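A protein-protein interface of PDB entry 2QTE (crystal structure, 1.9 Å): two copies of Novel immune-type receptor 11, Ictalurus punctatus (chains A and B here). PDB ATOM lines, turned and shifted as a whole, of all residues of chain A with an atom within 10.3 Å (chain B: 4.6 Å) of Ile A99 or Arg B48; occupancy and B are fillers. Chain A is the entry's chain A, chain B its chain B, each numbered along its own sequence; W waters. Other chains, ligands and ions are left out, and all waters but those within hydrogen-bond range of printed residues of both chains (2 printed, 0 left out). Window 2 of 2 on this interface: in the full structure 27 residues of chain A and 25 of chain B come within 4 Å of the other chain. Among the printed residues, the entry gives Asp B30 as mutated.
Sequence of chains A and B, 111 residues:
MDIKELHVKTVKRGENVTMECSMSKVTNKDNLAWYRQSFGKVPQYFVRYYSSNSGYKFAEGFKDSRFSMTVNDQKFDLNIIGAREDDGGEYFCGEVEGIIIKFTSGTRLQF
Of the printed residues of chain A, Asp B30 touches Ile A99. Of chain A, only Ile A99 comes within 4 Å of Asn B31. No residue of chain A comes within 4 Å of Val B47. Arg B48 touches just one residue of chain A: Ile A99. Printed residues of chain A within 4 Å of Val B96: Val A96, Gly A98, Ile A99 and Ile A100.
Of the 15 printed residues of chain B, 6 touch a printed residue of chain A. Hydrophobic or aromatic side chains of chain B that line the printed part of chain A: Tyr B35, Tyr B45 and Val B96. Hydrophobic or aromatic side chains of chain A that line the printed part of chain B: Val A96, Ile A99, Ile A100 and Ile A101.
O of Asn A31 sits at hydrogen-bond distance from N of Val A96 (2.9 Å). O of Asn B31 is in hydrogen-bond range of N of Val B96. The guanidinium group (NE) of Arg B48 sits close to the side-chain hydroxyl (OH) of Tyr B45 (3.3 Å). O of Lys B57 lies within hydrogen-bond range of OH of Tyr B45, 3.5 Å away. O of Arg B48 lies within hydrogen-bond range of N of Lys B57 (3.0 Å).
Val A96 touches its own counterpart, Val B96. Positions printed for both chains: 31 and 96. Of the 10 pairs that touch across the chains among the printed residues, 1 has its exchanged pair printed and touching as well.
N of Ile A101 sits at hydrogen-bond distance from OH of Tyr B35.
CG1 of Val A96 touches CG1 of Val B96, at 3.7 Å. Val B96 touches Gly A98. O of Asp B30 touches CD1 of Ile A99 (2.9 Å). OD1 of Asn B31 touches CG2 of Ile A99, at 2.9 Å. NH2 of Arg B48 touches CD1 of Ile A99, 3.7 Å away. Ile A99 touches Val B96. Tyr B35 touches Ile A100. Tyr B45 touches Ile A100 (CG to CG1, 3.4 Å). Val B96 touches Ile A100.
Water W1 bridges the backbone carbonyl oxygen of Ile A101 (2.7 Å) and the backbone NH of Tyr B45 (3.1 Å). Water W2 lies within hydrogen-bond range of the backbone carbonyl oxygen (O) of Asn B31 and the backbone carbonyl oxygen (O) of Ile A99.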
ATOM      1  N   ASN A  31      33.729   0.604  13.991  1.00  0.00           N
ATOM      2  CA  ASN A  31      32.543   0.125  13.257  1.00  0.00           C
ATOM      3  C   ASN A  31      32.144   1.070  12.140  1.00  0.00           C
ATOM      4  O   ASN A  31      30.972   1.113  11.716  1.00  0.00           O
ATOM      5  CB  ASN A  31      31.339  -0.125  14.186  1.00  0.00           C
ATOM      6  CG  ASN A  31      31.630  -1.153  15.263  1.00  0.00           C
ATOM      7  OD1 ASN A  31      32.775  -1.394  15.595  1.00  0.00           O
ATOM      8  ND2 ASN A  31      30.586  -1.745  15.827  1.00  0.00           N
ATOM      9  N   GLU A  95      28.119   3.971  10.406  1.00  0.00           N
ATOM     10  CA  GLU A  95      28.698   3.380  11.592  1.00  0.00           C
ATOM     11  C   GLU A  95      27.734   2.367  12.217  1.00  0.00           C
ATOM     12  O   GLU A  95      26.585   2.708  12.443  1.00  0.00           O
ATOM     13  CB  GLU A  95      28.985   4.530  12.561  1.00  0.00           C
ATOM     14  CG  GLU A  95      29.870   4.130  13.675  1.00  0.00           C
ATOM     15  CD  GLU A  95      29.962   5.162  14.773  1.00  0.00           C
ATOM     16  OE1 GLU A  95      29.842   6.373  14.503  1.00  0.00           O
ATOM     17  OE2 GLU A  95      30.164   4.720  15.913  1.00  0.00           O
ATOM     18  N   VAL A  96      28.175   1.119  12.450  1.00  0.00           N
ATOM     19  CA  VAL A  96      27.356   0.109  13.162  1.00  0.00           C
ATOM     20  C   VAL A  96      27.279   0.498  14.643  1.00  0.00           C
ATOM     21  O   VAL A  96      28.302   0.731  15.276  1.00  0.00           O
ATOM     22  CB  VAL A  96      27.865  -1.350  12.997  1.00  0.00           C
ATOM     23  CG1 VAL A  96      27.283  -2.311  14.075  1.00  0.00           C
ATOM     24  CG2 VAL A  96      27.576  -1.873  11.604  1.00  0.00           C
ATOM     25  N   GLU A  97      26.051   0.605  15.154  1.00  0.00           N
ATOM     26  CA  GLU A  97      25.799   0.961  16.559  1.00  0.00           C
ATOM     27  C   GLU A  97      24.756   0.032  17.164  1.00  0.00           C
ATOM     28  O   GLU A  97      23.586   0.253  17.022  1.00  0.00           O
ATOM     29  CB  GLU A  97      25.335   2.408  16.655  1.00  0.00           C
ATOM     30  CG  GLU A  97      26.229   3.282  17.552  1.00  0.00           C
ATOM     31  CD  GLU A  97      25.727   3.420  18.986  1.00  0.00           C
ATOM     32  OE1 GLU A  97      24.751   2.718  19.361  1.00  0.00           O
ATOM     33  OE2 GLU A  97      26.302   4.248  19.740  1.00  0.00           O
ATOM     34  N   GLY A  98      25.203  -1.030  17.819  1.00  0.00           N
ATOM     35  CA  GLY A  98      24.294  -2.029  18.348  1.00  0.00           C
ATOM     36  C   GLY A  98      23.871  -2.958  17.234  1.00  0.00           C
ATOM     37  O   GLY A  98      24.711  -3.430  16.470  1.00  0.00           O
ATOM     38  N   ILE A  99      22.574  -3.213  17.123  1.00  0.00           N
ATOM     39  CA  ILE A  99      22.067  -4.125  16.096  1.00  0.00           C
ATOM     40  C   ILE A  99      21.637  -3.371  14.822  1.00  0.00           C
ATOM     41  O   ILE A  99      20.990  -3.960  13.936  1.00  0.00           O
ATOM     42  CB  ILE A  99      20.925  -4.997  16.655  1.00  0.00           C
ATOM     43  CG1 ILE A  99      19.718  -4.143  17.101  1.00  0.00           C
ATOM     44  CG2 ILE A  99      21.451  -5.840  17.837  1.00  0.00           C
ATOM     45  CD1 ILE A  99      18.469  -4.919  17.466  1.00  0.00           C
ATOM     46  N   ILE A 100      22.045  -2.096  14.741  1.00  0.00           N
ATOM     47  CA  ILE A 100      21.652  -1.149  13.693  1.00  0.00           C
ATOM     48  C   ILE A 100      22.884  -0.410  13.170  1.00  0.00           C
ATOM     49  O   ILE A 100      23.871  -0.364  13.863  1.00  0.00           O
ATOM     50  CB  ILE A 100      20.499  -0.207  14.228  1.00  0.00           C
ATOM     51  CG1 ILE A 100      19.180  -0.590  13.571  1.00  0.00           C
ATOM     52  CG2 ILE A 100      20.772   1.300  14.024  1.00  0.00           C
ATOM     53  CD1 ILE A 100      18.565  -1.890  14.078  1.00  0.00           C
ATOM     54  N   ILE A 101      22.838   0.084  11.921  1.00  0.00           N
ATOM     55  CA  ILE A 101      23.855   0.989  11.343  1.00  0.00           C
ATOM     56  C   ILE A 101      23.208   2.326  10.972  1.00  0.00           C
ATOM     57  O   ILE A 101      22.078   2.356  10.471  1.00  0.00           O
ATOM     58  CB  ILE A 101      24.627   0.343  10.100  1.00  0.00           C
ATOM     59  CG1 ILE A 101      25.748   1.278   9.569  1.00  0.00           C
ATOM     60  CG2 ILE A 101      23.661  -0.112   8.991  1.00  0.00           C
ATOM     61  CD1 ILE A 101      25.314   2.530   8.800  1.00  0.00           C
ATOM     62  N   LYS A 102      23.896   3.428  11.272  1.00  0.00           N
ATOM     63  CA  LYS A 102      23.461   4.764  10.899  1.00  0.00           C
ATOM     64  C   LYS A 102      24.408   5.323   9.835  1.00  0.00           C
ATOM     65  O   LYS A 102      25.603   5.373  10.059  1.00  0.00           O
ATOM     66  CB  LYS A 102      23.459   5.705  12.127  1.00  0.00           C
ATOM     67  CG  LYS A 102      22.449   5.303  13.168  1.00  0.00           C
ATOM     68  CD  LYS A 102      21.843   6.518  13.889  1.00  0.00           C
ATOM     69  CE  LYS A 102      22.455   6.706  15.275  1.00  0.00           C
ATOM     70  NZ  LYS A 102      21.523   7.378  16.288  1.00  0.00           N
ATOM     71  N   ASP B  30      17.797 -11.039  16.130  1.00  0.00           N
ATOM     72  CA  ASP B  30      17.777  -9.750  16.797  1.00  0.00           C
ATOM     73  C   ASP B  30      18.488  -8.671  15.999  1.00  0.00           C
ATOM     74  O   ASP B  30      18.149  -7.490  16.104  1.00  0.00           O
ATOM     75  CB  ASP B  30      18.435  -9.906  18.152  1.00  0.00           C
ATOM     76  CG  ASP B  30      17.650 -10.863  19.051  1.00  0.00           C
ATOM     77  OD1 ASP B  30      16.421 -10.999  18.815  1.00  0.00           O
ATOM     78  OD2 ASP B  30      18.252 -11.474  19.963  1.00  0.00           O
ATOM     79  N   ASN B  31      19.450  -9.116  15.189  1.00  0.00           N
ATOM     80  CA  ASN B  31      20.290  -8.257  14.336  1.00  0.00           C
ATOM     81  C   ASN B  31      19.737  -7.956  12.954  1.00  0.00           C
ATOM     82  O   ASN B  31      20.443  -7.359  12.133  1.00  0.00           O
ATOM     83  CB  ASN B  31      21.675  -8.900  14.158  1.00  0.00           C
ATOM     84  CG  ASN B  31      22.457  -8.951  15.445  1.00  0.00           C
ATOM     85  OD1 ASN B  31      22.265  -8.115  16.321  1.00  0.00           O
ATOM     86  ND2 ASN B  31      23.340  -9.938  15.570  1.00  0.00           N
ATOM     87  N   LEU B  32      18.480  -8.346  12.697  1.00  0.00           N
ATOM     88  CA  LEU B  32      17.919  -8.304  11.349  1.00  0.00           C
ATOM     89  C   LEU B  32      16.993  -7.130  11.297  1.00  0.00           C
ATOM     90  O   LEU B  32      16.285  -6.851  12.258  1.00  0.00           O
ATOM     91  CB  LEU B  32      17.187  -9.615  11.053  1.00  0.00           C
ATOM     92  CG  LEU B  32      16.555  -9.966   9.720  1.00  0.00           C
ATOM     93  CD1 LEU B  32      17.625 -10.231   8.669  1.00  0.00           C
ATOM     94  CD2 LEU B  32      15.773 -11.239   9.996  1.00  0.00           C
ATOM     95  N   ALA B  33      17.042  -6.410  10.163  1.00  0.00           N
ATOM     96  CA  ALA B  33      16.303  -5.194   9.964  1.00  0.00           C
ATOM     97  C   ALA B  33      16.171  -4.874   8.483  1.00  0.00           C
ATOM     98  O   ALA B  33      16.996  -5.284   7.692  1.00  0.00           O
ATOM     99  CB  ALA B  33      17.022  -4.072  10.633  1.00  0.00           C
ATOM    100  N   TYR B  35      16.050  -1.628   5.824  1.00  0.00           N
ATOM    101  CA  TYR B  35      16.540  -0.233   5.693  1.00  0.00           C
ATOM    102  C   TYR B  35      15.821   0.393   4.552  1.00  0.00           C
ATOM    103  O   TYR B  35      15.506  -0.295   3.578  1.00  0.00           O
ATOM    104  CB  TYR B  35      18.049  -0.222   5.463  1.00  0.00           C
ATOM    105  CG  TYR B  35      18.774  -0.554   6.745  1.00  0.00           C
ATOM    106  CD1 TYR B  35      18.715  -1.859   7.307  1.00  0.00           C
ATOM    107  CD2 TYR B  35      19.468   0.446   7.437  1.00  0.00           C
ATOM    108  CE1 TYR B  35      19.369  -2.151   8.501  1.00  0.00           C
ATOM    109  CE2 TYR B  35      20.112   0.170   8.631  1.00  0.00           C
ATOM    110  CZ  TYR B  35      20.044  -1.116   9.158  1.00  0.00           C
ATOM    111  OH  TYR B  35      20.678  -1.356  10.327  1.00  0.00           O
ATOM    112  N   TYR B  45      17.632   2.899   8.827  1.00  0.00           N
ATOM    113  CA  TYR B  45      17.025   1.769   9.530  1.00  0.00           C
ATOM    114  C   TYR B  45      15.544   2.018   9.604  1.00  0.00           C
ATOM    115  O   TYR B  45      15.110   3.124   9.961  1.00  0.00           O
ATOM    116  CB  TYR B  45      17.610   1.667  10.946  1.00  0.00           C
ATOM    117  CG  TYR B  45      16.682   1.129  11.996  1.00  0.00           C
ATOM    118  CD1 TYR B  45      16.068  -0.116  11.832  1.00  0.00           C
ATOM    119  CD2 TYR B  45      16.437   1.831  13.172  1.00  0.00           C
ATOM    120  CE1 TYR B  45      15.205  -0.631  12.780  1.00  0.00           C
ATOM    121  CE2 TYR B  45      15.557   1.307  14.167  1.00  0.00           C
ATOM    122  CZ  TYR B  45      14.963   0.058  13.942  1.00  0.00           C
ATOM    123  OH  TYR B  45      14.101  -0.528  14.859  1.00  0.00           O
ATOM    124  N   VAL B  47      12.805  -0.839  10.402  1.00  0.00           N
ATOM    125  CA  VAL B  47      11.994  -1.788  11.198  1.00  0.00           C
ATOM    126  C   VAL B  47      12.914  -2.984  11.459  1.00  0.00           C
ATOM    127  O   VAL B  47      13.669  -3.425  10.567  1.00  0.00           O
ATOM    128  CB  VAL B  47      10.664  -2.197  10.519  1.00  0.00           C
ATOM    129  CG1 VAL B  47      10.914  -2.822   9.127  1.00  0.00           C
ATOM    130  CG2 VAL B  47       9.820  -3.193  11.408  1.00  0.00           C
ATOM    131  N   ARG B  48      12.919  -3.460  12.703  1.00  0.00           N
ATOM    132  CA  ARG B  48      13.802  -4.559  13.064  1.00  0.00           C
ATOM    133  C   ARG B  48      13.011  -5.717  13.586  1.00  0.00           C
ATOM    134  O   ARG B  48      11.885  -5.540  13.985  1.00  0.00           O
ATOM    135  CB  ARG B  48      14.744  -4.140  14.189  1.00  0.00           C
ATOM    136  CG  ARG B  48      14.062  -3.563  15.423  1.00  0.00           C
ATOM    137  CD  ARG B  48      15.155  -3.049  16.315  1.00  0.00           C
ATOM    138  NE  ARG B  48      14.665  -2.410  17.525  1.00  0.00           N
ATOM    139  CZ  ARG B  48      14.685  -2.981  18.720  1.00  0.00           C
ATOM    140  NH1 ARG B  48      14.230  -2.309  19.779  1.00  0.00           N
ATOM    141  NH2 ARG B  48      15.158  -4.220  18.861  1.00  0.00           N
ATOM    142  N   TYR B  49      13.600  -6.904  13.566  1.00  0.00           N
ATOM    143  CA  TYR B  49      13.037  -8.025  14.259  1.00  0.00           C
ATOM    144  C   TYR B  49      12.933  -7.649  15.748  1.00  0.00           C
ATOM    145  O   TYR B  49      13.865  -6.990  16.275  1.00  0.00           O
ATOM    146  CB  TYR B  49      13.955  -9.226  14.109  1.00  0.00           C
ATOM    147  CG  TYR B  49      13.427 -10.432  14.837  1.00  0.00           C
ATOM    148  CD1 TYR B  49      13.645 -10.577  16.221  1.00  0.00           C
ATOM    149  CD2 TYR B  49      12.639 -11.388  14.175  1.00  0.00           C
ATOM    150  CE1 TYR B  49      13.142 -11.675  16.909  1.00  0.00           C
ATOM    151  CE2 TYR B  49      12.119 -12.454  14.856  1.00  0.00           C
ATOM    152  CZ  TYR B  49      12.379 -12.615  16.210  1.00  0.00           C
ATOM    153  OH  TYR B  49      11.847 -13.712  16.885  1.00  0.00           O
ATOM    154  N   TYR B  50      11.838  -8.046  16.423  1.00  0.00           N
ATOM    155  CA  TYR B  50      11.759  -7.866  17.867  1.00  0.00           C
ATOM    156  C   TYR B  50      10.932  -8.968  18.517  1.00  0.00           C
ATOM    157  O   TYR B  50       9.837  -9.224  18.076  1.00  0.00           O
ATOM    158  CB  TYR B  50      11.138  -6.504  18.148  1.00  0.00           C
ATOM    159  CG  TYR B  50      11.163  -6.045  19.592  1.00  0.00           C
ATOM    160  CD1 TYR B  50       9.983  -5.969  20.332  1.00  0.00           C
ATOM    161  CD2 TYR B  50      12.335  -5.593  20.179  1.00  0.00           C
ATOM    162  CE1 TYR B  50       9.983  -5.502  21.656  1.00  0.00           C
ATOM    163  CE2 TYR B  50      12.356  -5.105  21.486  1.00  0.00           C
ATOM    164  CZ  TYR B  50      11.169  -5.065  22.222  1.00  0.00           C
ATOM    165  OH  TYR B  50      11.165  -4.583  23.516  1.00  0.00           O
ATOM    166  N   GLY B  55       6.426  -9.609  16.363  1.00  0.00           N
ATOM    167  CA  GLY B  55       7.701 -10.049  15.837  1.00  0.00           C
ATOM    168  C   GLY B  55       8.553  -8.898  15.301  1.00  0.00           C
ATOM    169  O   GLY B  55       9.635  -9.131  14.855  1.00  0.00           O
ATOM    170  N   TYR B  56       8.111  -7.647  15.382  1.00  0.00           N
ATOM    171  CA  TYR B  56       8.910  -6.560  14.814  1.00  0.00           C
ATOM    172  C   TYR B  56       8.649  -5.267  15.516  1.00  0.00           C
ATOM    173  O   TYR B  56       7.637  -5.134  16.183  1.00  0.00           O
ATOM    174  CB  TYR B  56       8.618  -6.338  13.328  1.00  0.00           C
ATOM    175  CG  TYR B  56       7.165  -6.053  12.970  1.00  0.00           C
ATOM    176  CD1 TYR B  56       6.694  -4.727  12.845  1.00  0.00           C
ATOM    177  CD2 TYR B  56       6.254  -7.112  12.758  1.00  0.00           C
ATOM    178  CE1 TYR B  56       5.379  -4.478  12.548  1.00  0.00           C
ATOM    179  CE2 TYR B  56       4.945  -6.882  12.443  1.00  0.00           C
ATOM    180  CZ  TYR B  56       4.503  -5.569  12.330  1.00  0.00           C
ATOM    181  OH  TYR B  56       3.208  -5.351  11.981  1.00  0.00           O
ATOM    182  N   LYS B  57       9.488  -4.287  15.249  1.00  0.00           N
ATOM    183  CA  LYS B  57       9.276  -2.981  15.814  1.00  0.00           C
ATOM    184  C   LYS B  57       9.809  -1.927  14.841  1.00  0.00           C
ATOM    185  O   LYS B  57      10.950  -1.986  14.453  1.00  0.00           O
ATOM    186  CB  LYS B  57      10.011  -2.913  17.138  1.00  0.00           C
ATOM    187  CG  LYS B  57       9.733  -1.635  17.926  1.00  0.00           C
ATOM    188  CD  LYS B  57      10.287  -1.795  19.304  1.00  0.00           C
ATOM    189  CE  LYS B  57      10.190  -0.468  19.975  1.00  0.00           C
ATOM    190  NZ  LYS B  57      10.983   0.533  19.189  1.00  0.00           N
ATOM    191  N   PHE B  76      10.602 -12.793   6.987  1.00  0.00           N
ATOM    192  CA  PHE B  76      10.757 -11.471   7.618  1.00  0.00           C
ATOM    193  C   PHE B  76      10.340 -10.496   6.500  1.00  0.00           C
ATOM    194  O   PHE B  76      11.168  -9.756   5.986  1.00  0.00           O
ATOM    195  CB  PHE B  76      12.218 -11.263   8.030  1.00  0.00           C
ATOM    196  CG  PHE B  76      12.515  -9.954   8.759  1.00  0.00           C
ATOM    197  CD1 PHE B  76      12.043  -9.705  10.049  1.00  0.00           C
ATOM    198  CD2 PHE B  76      13.341  -9.009   8.172  1.00  0.00           C
ATOM    199  CE1 PHE B  76      12.356  -8.556  10.707  1.00  0.00           C
ATOM    200  CE2 PHE B  76      13.679  -7.809   8.856  1.00  0.00           C
ATOM    201  CZ  PHE B  76      13.177  -7.577  10.105  1.00  0.00           C
ATOM    202  N   VAL B  96      23.167  -7.203  10.916  1.00  0.00           N
ATOM    203  CA  VAL B  96      24.462  -6.757  11.425  1.00  0.00           C
ATOM    204  C   VAL B  96      25.237  -8.006  11.851  1.00  0.00           C
ATOM    205  O   VAL B  96      24.718  -8.874  12.570  1.00  0.00           O
ATOM    206  CB  VAL B  96      24.355  -5.714  12.586  1.00  0.00           C
ATOM    207  CG1 VAL B  96      25.700  -5.550  13.262  1.00  0.00           C
ATOM    208  CG2 VAL B  96      23.877  -4.347  12.087  1.00  0.00           C
HETATM  209  O   HOH W   1      20.061   4.166  10.177  1.00  0.00           O
HETATM  210  O   HOH W   2      20.371  -4.776  11.170  1.00  0.00           O
